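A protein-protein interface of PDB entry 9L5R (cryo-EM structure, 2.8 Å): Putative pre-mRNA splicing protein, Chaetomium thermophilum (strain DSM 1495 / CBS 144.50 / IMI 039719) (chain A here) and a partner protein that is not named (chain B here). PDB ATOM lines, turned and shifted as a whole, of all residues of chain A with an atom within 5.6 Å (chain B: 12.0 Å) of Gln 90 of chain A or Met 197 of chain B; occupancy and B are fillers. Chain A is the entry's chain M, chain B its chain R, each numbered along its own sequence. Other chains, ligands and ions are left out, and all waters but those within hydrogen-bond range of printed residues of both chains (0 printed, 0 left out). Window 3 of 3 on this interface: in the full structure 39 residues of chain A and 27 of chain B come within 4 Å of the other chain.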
ATOM      1  N   CYS A  23     -15.896 -14.243  24.576  1.00  0.00           N
ATOM      2  CA  CYS A  23     -16.425 -12.960  24.155  1.00  0.00           C
ATOM      3  C   CYS A  23     -17.840 -13.097  23.607  1.00  0.00           C
ATOM      4  O   CYS A  23     -18.325 -14.192  23.324  1.00  0.00           O
ATOM      5  CB  CYS A  23     -15.518 -12.343  23.104  1.00  0.00           C
ATOM      6  SG  CYS A  23     -15.506 -13.177  21.509  1.00  0.00           S
ATOM      7  N   ASN A  25     -19.262 -12.235  20.783  1.00  0.00           N
ATOM      8  CA  ASN A  25     -19.519 -12.710  19.433  1.00  0.00           C
ATOM      9  C   ASN A  25     -19.335 -14.213  19.324  1.00  0.00           C
ATOM     10  O   ASN A  25     -19.978 -14.851  18.485  1.00  0.00           O
ATOM     11  CB  ASN A  25     -18.617 -11.992  18.437  1.00  0.00           C
ATOM     12  CG  ASN A  25     -19.234 -10.722  17.917  1.00  0.00           C
ATOM     13  OD1 ASN A  25     -20.052 -10.097  18.588  1.00  0.00           O
ATOM     14  ND2 ASN A  25     -18.849 -10.333  16.711  1.00  0.00           N
ATOM     15  N   ASN A  80      -4.240 -12.290  27.174  1.00  0.00           N
ATOM     16  CA  ASN A  80      -5.424 -11.427  27.116  1.00  0.00           C
ATOM     17  C   ASN A  80      -6.329 -11.779  25.939  1.00  0.00           C
ATOM     18  O   ASN A  80      -6.755 -10.916  25.172  1.00  0.00           O
ATOM     19  CB  ASN A  80      -5.037  -9.952  27.079  1.00  0.00           C
ATOM     20  CG  ASN A  80      -6.088  -9.070  27.694  1.00  0.00           C
ATOM     21  OD1 ASN A  80      -6.813  -9.485  28.589  1.00  0.00           O
ATOM     22  ND2 ASN A  80      -6.209  -7.858  27.186  1.00  0.00           N
ATOM     23  N   CYS A  82      -9.573 -14.105  23.958  1.00  0.00           N
ATOM     24  CA  CYS A  82     -10.808 -14.849  24.126  1.00  0.00           C
ATOM     25  C   CYS A  82     -10.496 -16.331  24.103  1.00  0.00           C
ATOM     26  O   CYS A  82      -9.607 -16.794  23.389  1.00  0.00           O
ATOM     27  CB  CYS A  82     -11.836 -14.539  23.044  1.00  0.00           C
ATOM     28  SG  CYS A  82     -13.197 -15.752  23.006  1.00  0.00           S
ATOM     29  N   CYS A  85     -12.100 -17.876  20.367  1.00  0.00           N
ATOM     30  CA  CYS A  85     -11.595 -17.368  19.097  1.00  0.00           C
ATOM     31  C   CYS A  85     -10.095 -17.132  19.097  1.00  0.00           C
ATOM     32  O   CYS A  85      -9.506 -17.041  18.016  1.00  0.00           O
ATOM     33  CB  CYS A  85     -12.295 -16.060  18.732  1.00  0.00           C
ATOM     34  SG  CYS A  85     -12.247 -14.834  20.033  1.00  0.00           S
ATOM     35  N   MET A  87      -8.656 -14.436  20.090  1.00  0.00           N
ATOM     36  CA  MET A  87      -8.369 -13.080  19.662  1.00  0.00           C
ATOM     37  C   MET A  87      -8.260 -12.169  20.873  1.00  0.00           C
ATOM     38  O   MET A  87      -8.823 -12.441  21.934  1.00  0.00           O
ATOM     39  CB  MET A  87      -9.404 -12.513  18.675  1.00  0.00           C
ATOM     40  CG  MET A  87      -9.607 -13.326  17.414  1.00  0.00           C
ATOM     41  SD  MET A  87     -10.875 -12.692  16.296  1.00  0.00           S
ATOM     42  CE  MET A  87     -12.342 -12.634  17.302  1.00  0.00           C
ATOM     43  N   ASP A  88      -7.499 -11.092  20.691  1.00  0.00           N
ATOM     44  CA  ASP A  88      -7.193 -10.147  21.758  1.00  0.00           C
ATOM     45  C   ASP A  88      -8.455  -9.491  22.291  1.00  0.00           C
ATOM     46  O   ASP A  88      -9.267  -8.978  21.525  1.00  0.00           O
ATOM     47  CB  ASP A  88      -6.237  -9.086  21.221  1.00  0.00           C
ATOM     48  CG  ASP A  88      -6.092  -7.904  22.146  1.00  0.00           C
ATOM     49  OD1 ASP A  88      -5.803  -8.100  23.346  1.00  0.00           O
ATOM     50  OD2 ASP A  88      -6.270  -6.770  21.667  1.00  0.00           O
ATOM     51  N   LEU A  89      -8.599  -9.474  23.613  1.00  0.00           N
ATOM     52  CA  LEU A  89      -9.827  -9.006  24.239  1.00  0.00           C
ATOM     53  C   LEU A  89      -9.985  -7.496  24.218  1.00  0.00           C
ATOM     54  O   LEU A  89     -11.035  -7.002  24.635  1.00  0.00           O
ATOM     55  CB  LEU A  89      -9.905  -9.493  25.683  1.00  0.00           C
ATOM     56  CG  LEU A  89     -10.317 -10.947  25.896  1.00  0.00           C
ATOM     57  CD1 LEU A  89     -10.384 -11.259  27.367  1.00  0.00           C
ATOM     58  CD2 LEU A  89     -11.641 -11.211  25.237  1.00  0.00           C
ATOM     59  N   GLN A  90      -8.986  -6.747  23.756  1.00  0.00           N
ATOM     60  CA  GLN A  90      -9.075  -5.297  23.765  1.00  0.00           C
ATOM     61  C   GLN A  90      -9.306  -4.674  22.398  1.00  0.00           C
ATOM     62  O   GLN A  90      -9.803  -3.549  22.342  1.00  0.00           O
ATOM     63  CB  GLN A  90      -7.810  -4.689  24.386  1.00  0.00           C
ATOM     64  CG  GLN A  90      -7.824  -4.719  25.899  1.00  0.00           C
ATOM     65  CD  GLN A  90      -6.592  -4.096  26.521  1.00  0.00           C
ATOM     66  OE1 GLN A  90      -5.464  -4.392  26.130  1.00  0.00           O
ATOM     67  NE2 GLN A  90      -6.803  -3.235  27.508  1.00  0.00           N
ATOM     68  N   PHE A  91      -8.970  -5.363  21.302  1.00  0.00           N
ATOM     69  CA  PHE A  91      -9.143  -4.804  19.964  1.00  0.00           C
ATOM     70  C   PHE A  91      -9.734  -5.751  18.940  1.00  0.00           C
ATOM     71  O   PHE A  91     -10.151  -5.278  17.878  1.00  0.00           O
ATOM     72  CB  PHE A  91      -7.806  -4.295  19.411  1.00  0.00           C
ATOM     73  CG  PHE A  91      -7.123  -3.332  20.310  1.00  0.00           C
ATOM     74  CD1 PHE A  91      -7.716  -2.128  20.633  1.00  0.00           C
ATOM     75  CD2 PHE A  91      -5.904  -3.647  20.864  1.00  0.00           C
ATOM     76  CE1 PHE A  91      -7.101  -1.263  21.482  1.00  0.00           C
ATOM     77  CE2 PHE A  91      -5.285  -2.782  21.707  1.00  0.00           C
ATOM     78  CZ  PHE A  91      -5.885  -1.597  22.021  1.00  0.00           C
ATOM     79  N   GLY A  92      -9.782  -7.053  19.198  1.00  0.00           N
ATOM     80  CA  GLY A  92     -10.273  -7.974  18.193  1.00  0.00           C
ATOM     81  C   GLY A  92      -9.251  -8.378  17.170  1.00  0.00           C
ATOM     82  O   GLY A  92      -9.589  -8.557  15.998  1.00  0.00           O
ATOM     83  N   LEU A  93      -8.018  -8.505  17.571  1.00  0.00           N
ATOM     84  CA  LEU A  93      -6.944  -8.887  16.694  1.00  0.00           C
ATOM     85  C   LEU A  93      -6.499 -10.304  17.010  1.00  0.00           C
ATOM     86  O   LEU A  93      -6.701 -10.778  18.128  1.00  0.00           O
ATOM     87  CB  LEU A  93      -5.747  -7.944  16.854  1.00  0.00           C
ATOM     88  CG  LEU A  93      -5.842  -6.529  16.292  1.00  0.00           C
ATOM     89  CD1 LEU A  93      -4.695  -5.692  16.813  1.00  0.00           C
ATOM     90  CD2 LEU A  93      -5.832  -6.570  14.782  1.00  0.00           C
ATOM     91  N   ARG A  98      -1.565  -8.547  17.318  1.00  0.00           N
ATOM     92  CA  ARG A  98      -1.580  -7.588  18.419  1.00  0.00           C
ATOM     93  C   ARG A  98      -0.191  -7.437  19.014  1.00  0.00           C
ATOM     94  O   ARG A  98       0.307  -6.321  19.178  1.00  0.00           O
ATOM     95  CB  ARG A  98      -2.574  -8.045  19.496  1.00  0.00           C
ATOM     96  CG  ARG A  98      -2.890  -7.058  20.654  1.00  0.00           C
ATOM     97  CD  ARG A  98      -1.902  -7.084  21.827  1.00  0.00           C
ATOM     98  NE  ARG A  98      -1.697  -8.396  22.431  1.00  0.00           N
ATOM     99  CZ  ARG A  98      -2.461  -8.932  23.371  1.00  0.00           C
ATOM    100  NH1 ARG A  98      -3.482  -8.276  23.891  1.00  0.00           N
ATOM    101  NH2 ARG A  98      -2.167 -10.143  23.828  1.00  0.00           N
ATOM    102  N   LYS A 138      -5.762  -0.815  29.882  1.00  0.00           N
ATOM    103  CA  LYS A 138      -5.299  -0.660  31.256  1.00  0.00           C
ATOM    104  C   LYS A 138      -3.768  -0.629  31.305  1.00  0.00           C
ATOM    105  O   LYS A 138      -3.171  -0.142  32.268  1.00  0.00           O
ATOM    106  CB  LYS A 138      -5.851  -1.787  32.134  1.00  0.00           C
ATOM    107  CG  LYS A 138      -7.371  -1.775  32.257  1.00  0.00           C
ATOM    108  CD  LYS A 138      -7.957  -3.182  32.347  1.00  0.00           C
ATOM    109  CE  LYS A 138      -9.450  -3.181  32.013  1.00  0.00           C
ATOM    110  NZ  LYS A 138      -9.929  -4.501  31.520  1.00  0.00           N
ATOM    111  N   THR A 139      -3.139  -1.156  30.252  1.00  0.00           N
ATOM    112  CA  THR A 139      -1.688  -1.216  30.160  1.00  0.00           C
ATOM    113  C   THR A 139      -1.133  -0.833  28.792  1.00  0.00           C
ATOM    114  O   THR A 139       0.080  -0.622  28.680  1.00  0.00           O
ATOM    115  CB  THR A 139      -1.192  -2.628  30.524  1.00  0.00           C
ATOM    116  OG1 THR A 139      -2.041  -3.613  29.922  1.00  0.00           O
ATOM    117  CG2 THR A 139      -1.187  -2.831  32.034  1.00  0.00           C
ATOM    118  N   ASP A 140      -1.972  -0.735  27.755  1.00  0.00           N
ATOM    119  CA  ASP A 140      -1.514  -0.610  26.378  1.00  0.00           C
ATOM    120  C   ASP A 140      -2.120   0.577  25.639  1.00  0.00           C
ATOM    121  O   ASP A 140      -1.981   0.656  24.408  1.00  0.00           O
ATOM    122  CB  ASP A 140      -1.815  -1.896  25.604  1.00  0.00           C
ATOM    123  CG  ASP A 140      -3.294  -2.159  25.474  1.00  0.00           C
ATOM    124  OD1 ASP A 140      -4.038  -1.836  26.419  1.00  0.00           O
ATOM    125  OD2 ASP A 140      -3.716  -2.691  24.432  1.00  0.00           O
ATOM    126  N   GLU A 141      -2.786   1.490  26.354  1.00  0.00           N
ATOM    127  CA  GLU A 141      -3.235   2.749  25.766  1.00  0.00           C
ATOM    128  C   GLU A 141      -2.076   3.505  25.142  1.00  0.00           C
ATOM    129  O   GLU A 141      -2.150   3.938  23.985  1.00  0.00           O
ATOM    130  CB  GLU A 141      -3.912   3.624  26.827  1.00  0.00           C
ATOM    131  CG  GLU A 141      -5.229   3.115  27.388  1.00  0.00           C
ATOM    132  CD  GLU A 141      -5.063   2.098  28.496  1.00  0.00           C
ATOM    133  OE1 GLU A 141      -3.913   1.818  28.893  1.00  0.00           O
ATOM    134  OE2 GLU A 141      -6.088   1.571  28.968  1.00  0.00           O
ATOM    135  N   ARG A 144      -0.859   1.740  21.847  1.00  0.00           N
ATOM    136  CA  ARG A 144      -1.478   1.991  20.550  1.00  0.00           C
ATOM    137  C   ARG A 144      -1.551   3.461  20.165  1.00  0.00           C
ATOM    138  O   ARG A 144      -1.598   3.756  18.959  1.00  0.00           O
ATOM    139  CB  ARG A 144      -2.847   1.333  20.378  1.00  0.00           C
ATOM    140  CG  ARG A 144      -4.116   1.816  21.055  1.00  0.00           C
ATOM    141  CD  ARG A 144      -4.372   1.423  22.477  1.00  0.00           C
ATOM    142  NE  ARG A 144      -5.760   1.781  22.765  1.00  0.00           N
ATOM    143  CZ  ARG A 144      -6.350   1.760  23.952  1.00  0.00           C
ATOM    144  NH1 ARG A 144      -5.855   1.060  24.956  1.00  0.00           N
ATOM    145  NH2 ARG A 144      -7.527   2.358  24.099  1.00  0.00           N
ATOM    146  N   TYR B 191     -24.063 -13.835  34.663  1.00  0.00           N
ATOM    147  CA  TYR B 191     -23.218 -13.231  33.623  1.00  0.00           C
ATOM    148  C   TYR B 191     -23.499 -11.803  33.160  1.00  0.00           C
ATOM    149  O   TYR B 191     -24.107 -11.604  32.105  1.00  0.00           O
ATOM    150  CB  TYR B 191     -23.136 -14.100  32.378  1.00  0.00           C
ATOM    151  CG  TYR B 191     -21.919 -13.708  31.562  1.00  0.00           C
ATOM    152  CD1 TYR B 191     -20.705 -13.426  32.183  1.00  0.00           C
ATOM    153  CD2 TYR B 191     -21.989 -13.582  30.188  1.00  0.00           C
ATOM    154  CE1 TYR B 191     -19.602 -13.052  31.453  1.00  0.00           C
ATOM    155  CE2 TYR B 191     -20.893 -13.213  29.457  1.00  0.00           C
ATOM    156  CZ  TYR B 191     -19.708 -12.946  30.092  1.00  0.00           C
ATOM    157  OH  TYR B 191     -18.625 -12.582  29.341  1.00  0.00           O
ATOM    158  N   PRO B 193     -21.831  -9.055  31.268  1.00  0.00           N
ATOM    159  CA  PRO B 193     -20.629  -8.922  30.441  1.00  0.00           C
ATOM    160  C   PRO B 193     -19.957  -7.565  30.596  1.00  0.00           C
ATOM    161  O   PRO B 193     -20.567  -6.573  30.996  1.00  0.00           O
ATOM    162  CB  PRO B 193     -21.159  -9.088  29.011  1.00  0.00           C
ATOM    163  CG  PRO B 193     -22.563  -9.544  29.145  1.00  0.00           C
ATOM    164  CD  PRO B 193     -23.047  -9.022  30.446  1.00  0.00           C
ATOM    165  N   SER B 194     -18.669  -7.541  30.258  1.00  0.00           N
ATOM    166  CA  SER B 194     -17.943  -6.307  29.988  1.00  0.00           C
ATOM    167  C   SER B 194     -18.188  -5.931  28.528  1.00  0.00           C
ATOM    168  O   SER B 194     -19.099  -6.470  27.895  1.00  0.00           O
ATOM    169  CB  SER B 194     -16.463  -6.463  30.338  1.00  0.00           C
ATOM    170  OG  SER B 194     -16.280  -6.586  31.736  1.00  0.00           O
ATOM    171  N   ALA B 195     -17.409  -5.000  27.977  1.00  0.00           N
ATOM    172  CA  ALA B 195     -17.862  -4.334  26.762  1.00  0.00           C
ATOM    173  C   ALA B 195     -17.846  -5.209  25.509  1.00  0.00           C
ATOM    174  O   ALA B 195     -18.904  -5.708  25.109  1.00  0.00           O
ATOM    175  CB  ALA B 195     -17.005  -3.090  26.525  1.00  0.00           C
ATOM    176  N   GLN B 196     -16.659  -5.471  24.951  1.00  0.00           N
ATOM    177  CA  GLN B 196     -16.463  -6.264  23.734  1.00  0.00           C
ATOM    178  C   GLN B 196     -14.956  -6.283  23.501  1.00  0.00           C
ATOM    179  O   GLN B 196     -14.210  -5.741  24.323  1.00  0.00           O
ATOM    180  CB  GLN B 196     -17.233  -5.672  22.534  1.00  0.00           C
ATOM    181  CG  GLN B 196     -17.349  -6.506  21.247  1.00  0.00           C
ATOM    182  CD  GLN B 196     -18.024  -7.849  21.465  1.00  0.00           C
ATOM    183  OE1 GLN B 196     -19.207  -7.911  21.798  1.00  0.00           O
ATOM    184  NE2 GLN B 196     -17.274  -8.935  21.270  1.00  0.00           N
ATOM    185  N   MET B 197     -14.481  -6.928  22.434  1.00  0.00           N
ATOM    186  CA  MET B 197     -13.147  -6.613  21.951  1.00  0.00           C
ATOM    187  C   MET B 197     -13.070  -5.141  21.576  1.00  0.00           C
ATOM    188  O   MET B 197     -12.433  -4.352  22.273  1.00  0.00           O
ATOM    189  CB  MET B 197     -12.755  -7.438  20.726  1.00  0.00           C
ATOM    190  CG  MET B 197     -12.348  -8.881  20.951  1.00  0.00           C
ATOM    191  SD  MET B 197     -13.620 -10.054  21.326  1.00  0.00           S
ATOM    192  CE  MET B 197     -14.379 -10.238  19.719  1.00  0.00           C
ATOM    193  N   GLY B 198     -13.761  -4.746  20.510  1.00  0.00           N
ATOM    194  CA  GLY B 198     -13.627  -3.406  19.977  1.00  0.00           C
ATOM    195  C   GLY B 198     -14.789  -2.467  20.201  1.00  0.00           C
ATOM    196  O   GLY B 198     -14.688  -1.289  19.834  1.00  0.00           O
ATOM    197  N   ASN B 199     -15.885  -2.926  20.795  1.00  0.00           N
ATOM    198  CA  ASN B 199     -17.080  -2.119  20.972  1.00  0.00           C
ATOM    199  C   ASN B 199     -17.226  -1.764  22.442  1.00  0.00           C
ATOM    200  O   ASN B 199     -16.965  -2.599  23.311  1.00  0.00           O
ATOM    201  CB  ASN B 199     -18.321  -2.863  20.480  1.00  0.00           C
ATOM    202  CG  ASN B 199     -18.349  -3.011  18.976  1.00  0.00           C
ATOM    203  OD1 ASN B 199     -18.020  -2.080  18.242  1.00  0.00           O
ATOM    204  ND2 ASN B 199     -18.738  -4.190  18.505  1.00  0.00           N
ATOM    205  N   ASN B 200     -17.618  -0.525  22.721  1.00  0.00           N
ATOM    206  CA  ASN B 200     -17.888  -0.108  24.087  1.00  0.00           C
ATOM    207  C   ASN B 200     -19.373   0.073  24.358  1.00  0.00           C
ATOM    208  O   ASN B 200     -19.744   0.541  25.438  1.00  0.00           O
ATOM    209  CB  ASN B 200     -17.119   1.170  24.413  1.00  0.00           C
ATOM    210  CG  ASN B 200     -15.661   0.899  24.712  1.00  0.00           C
ATOM    211  OD1 ASN B 200     -14.875   0.608  23.811  1.00  0.00           O
ATOM    212  ND2 ASN B 200     -15.292   0.977  25.984  1.00  0.00           N
ATOM    213  N   THR B 201     -20.225  -0.287  23.403  1.00  0.00           N
ATOM    214  CA  THR B 201     -21.660  -0.293  23.644  1.00  0.00           C
ATOM    215  C   THR B 201     -22.043  -1.416  24.602  1.00  0.00           C
ATOM    216  O   THR B 201     -21.489  -2.518  24.560  1.00  0.00           O
ATOM    217  CB  THR B 201     -22.423  -0.407  22.315  1.00  0.00           C
ATOM    218  OG1 THR B 201     -23.832  -0.297  22.551  1.00  0.00           O
ATOM    219  CG2 THR B 201     -22.105  -1.699  21.562  1.00  0.00           C
ATOM    220  N   LYS B 202     -22.966  -1.111  25.508  1.00  0.00           N
ATOM    221  CA  LYS B 202     -23.425  -2.090  26.478  1.00  0.00           C
ATOM    222  C   LYS B 202     -24.347  -3.085  25.786  1.00  0.00           C
ATOM    223  O   LYS B 202     -25.077  -2.740  24.853  1.00  0.00           O
ATOM    224  CB  LYS B 202     -24.133  -1.386  27.644  1.00  0.00           C
ATOM    225  CG  LYS B 202     -24.621  -2.269  28.799  1.00  0.00           C
ATOM    226  CD  LYS B 202     -26.078  -2.701  28.665  1.00  0.00           C
ATOM    227  CE  LYS B 202     -27.030  -1.544  28.868  1.00  0.00           C
ATOM    228  NZ  LYS B 202     -28.445  -1.993  28.743  1.00  0.00           N
ATOM    229  N   LYS B 203     -24.305  -4.333  26.243  1.00  0.00           N
ATOM    230  CA  LYS B 203     -25.155  -5.364  25.675  1.00  0.00           C
ATOM    231  C   LYS B 203     -25.644  -6.296  26.772  1.00  0.00           C
ATOM    232  O   LYS B 203     -25.236  -6.207  27.932  1.00  0.00           O
ATOM    233  CB  LYS B 203     -24.438  -6.112  24.548  1.00  0.00           C
ATOM    234  CG  LYS B 203     -23.047  -6.586  24.867  1.00  0.00           C
ATOM    235  CD  LYS B 203     -22.467  -7.245  23.637  1.00  0.00           C
ATOM    236  CE  LYS B 203     -22.373  -6.249  22.491  1.00  0.00           C
ATOM    237  NZ  LYS B 203     -21.793  -6.842  21.257  1.00  0.00           N
ATOM    238  N   ARG B 206     -26.671 -11.905  30.774  1.00  0.00           N
ATOM    239  CA  ARG B 206     -26.692 -13.273  30.263  1.00  0.00           C
ATOM    240  C   ARG B 206     -26.832 -14.310  31.368  1.00  0.00           C
ATOM    241  O   ARG B 206     -26.016 -14.358  32.304  1.00  0.00           O
ATOM    242  CB  ARG B 206     -25.435 -13.558  29.447  1.00  0.00           C
ATOM    243  CG  ARG B 206     -25.577 -13.238  27.994  1.00  0.00           C
ATOM    244  CD  ARG B 206     -24.566 -13.992  27.196  1.00  0.00           C
ATOM    245  NE  ARG B 206     -24.357 -13.394  25.889  1.00  0.00           N
ATOM    246  CZ  ARG B 206     -24.824 -13.906  24.763  1.00  0.00           C
ATOM    247  NH1 ARG B 206     -25.560 -14.998  24.760  1.00  0.00           N
ATOM    248  NH2 ARG B 206     -24.546 -13.309  23.611  1.00  0.00           N
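Along chain B the printed residues that touch a printed residue of chain A span positions 196 to 197.
Among the printed residues, no Asp or Glu carboxylate lies within 4 Å of a Lys or Arg side-chain nitrogen of the other chain.
Among the printed residues, pairs that only touch across the chains: Asn 25 of chain A with Gln 196 of chain B (3.9 Å), Met 87 of chain A with Met 197 of chain B (3.97 Å), Asp 88 of chain A with Met 197 of chain B (3.1 Å), Leu 89 of chain A with Met 197 of chain B (3.4 Å), Phe 91 of chain A with Met 197 of chain B (3.7 Å) and Gly 92 of chain A with Met 197 of chain B (3.4 Å).
The side-chain sulfur of Met 197 of chain B sits close to the side-chain sulfur of Cys 23 of chain A, at 3.7 Å.
The backbone carbonyl oxygen (O) of Gln 196 of chain B lies close to the backbone carbonyl oxygen (O) of Leu 89 of chain A.
The backbone carbonyl oxygen (O) of Met 197 of chain B sits close to the backbone carbonyl oxygen (O) of Gln 90 of chain A, 2.8 Å away.
Met 87 of chain A touches one residue of chain B.
Printed residues of chain B within 4 Å of Asp 88 of chain A: Met 197 (3.1 Å).
Leu 89 of chain A touches just these residues of chain B: Gln 196 and Met 197.
Gln 90 of chain A touches just one residue of chain B: Met 197 (2.8 Å).
Of chain B, only Met 197 (3.4 Å) comes within 4 Å of Gly 92 of chain A.
Lys 138 of chain A touches none of the printed residues of chain B.
No residue of chain B comes within 4 Å of Thr 139 of chain A.
No residue of chain B comes within 4 Å of Asp 140 of chain A.
Of the printed residues of chain A, Gln 196 of chain B touches Asn 25 and Leu 89.
Met 197 of chain B touches just these residues of chain A: Cys 23 (3.5 Å), Met 87 (3.97 Å), Asp 88 (3.1 Å), Leu 89 (3.4 Å), Gln 90 (2.8 Å), Phe 91 (3.7 Å) and Gly 92 (3.4 Å).
Lys 203 of chain B touches none of the printed residues of chain A.
The nearest residue of chain B that does not touch Gln 90 of chain A is Gly 198 of chain B (4.5 Å).
The nearest residue of chain A that does not touch Met 197 of chain B is Asn 25 of chain A (4.8 Å).
The nearest printed residue of chain A that does not touch Gln 196 of chain B is Cys 23 of chain A (4.2 Å).
The backbone carbonyl oxygen (O) of Asn 80 of chain A is in hydrogen-bond range of the backbone NH (N) of Leu 89 of chain A.
The backbone NH (N) of Cys 82 of chain A is in hydrogen-bond range of the backbone carbonyl oxygen (O) of Met 87 of chain A, at 2.7 Å.
The side-chain sulfur of Cys 85 of chain A lies close to the backbone NH of Met 87 of chain A (3.6 Å).
OD2 of Asp 88 of chain A is in hydrogen-bond range of N of Phe 91 of chain A.
OD2 of Asp 88 of chain A lies within salt-bridge range of NH1 of Arg 98 of chain A, 3.9 Å away.
The side-chain amide oxygen (OE1) of Gln 196 of chain B is in hydrogen-bond range of the side-chain amino group (NZ) of Lys 203 of chain B (2.9 Å).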
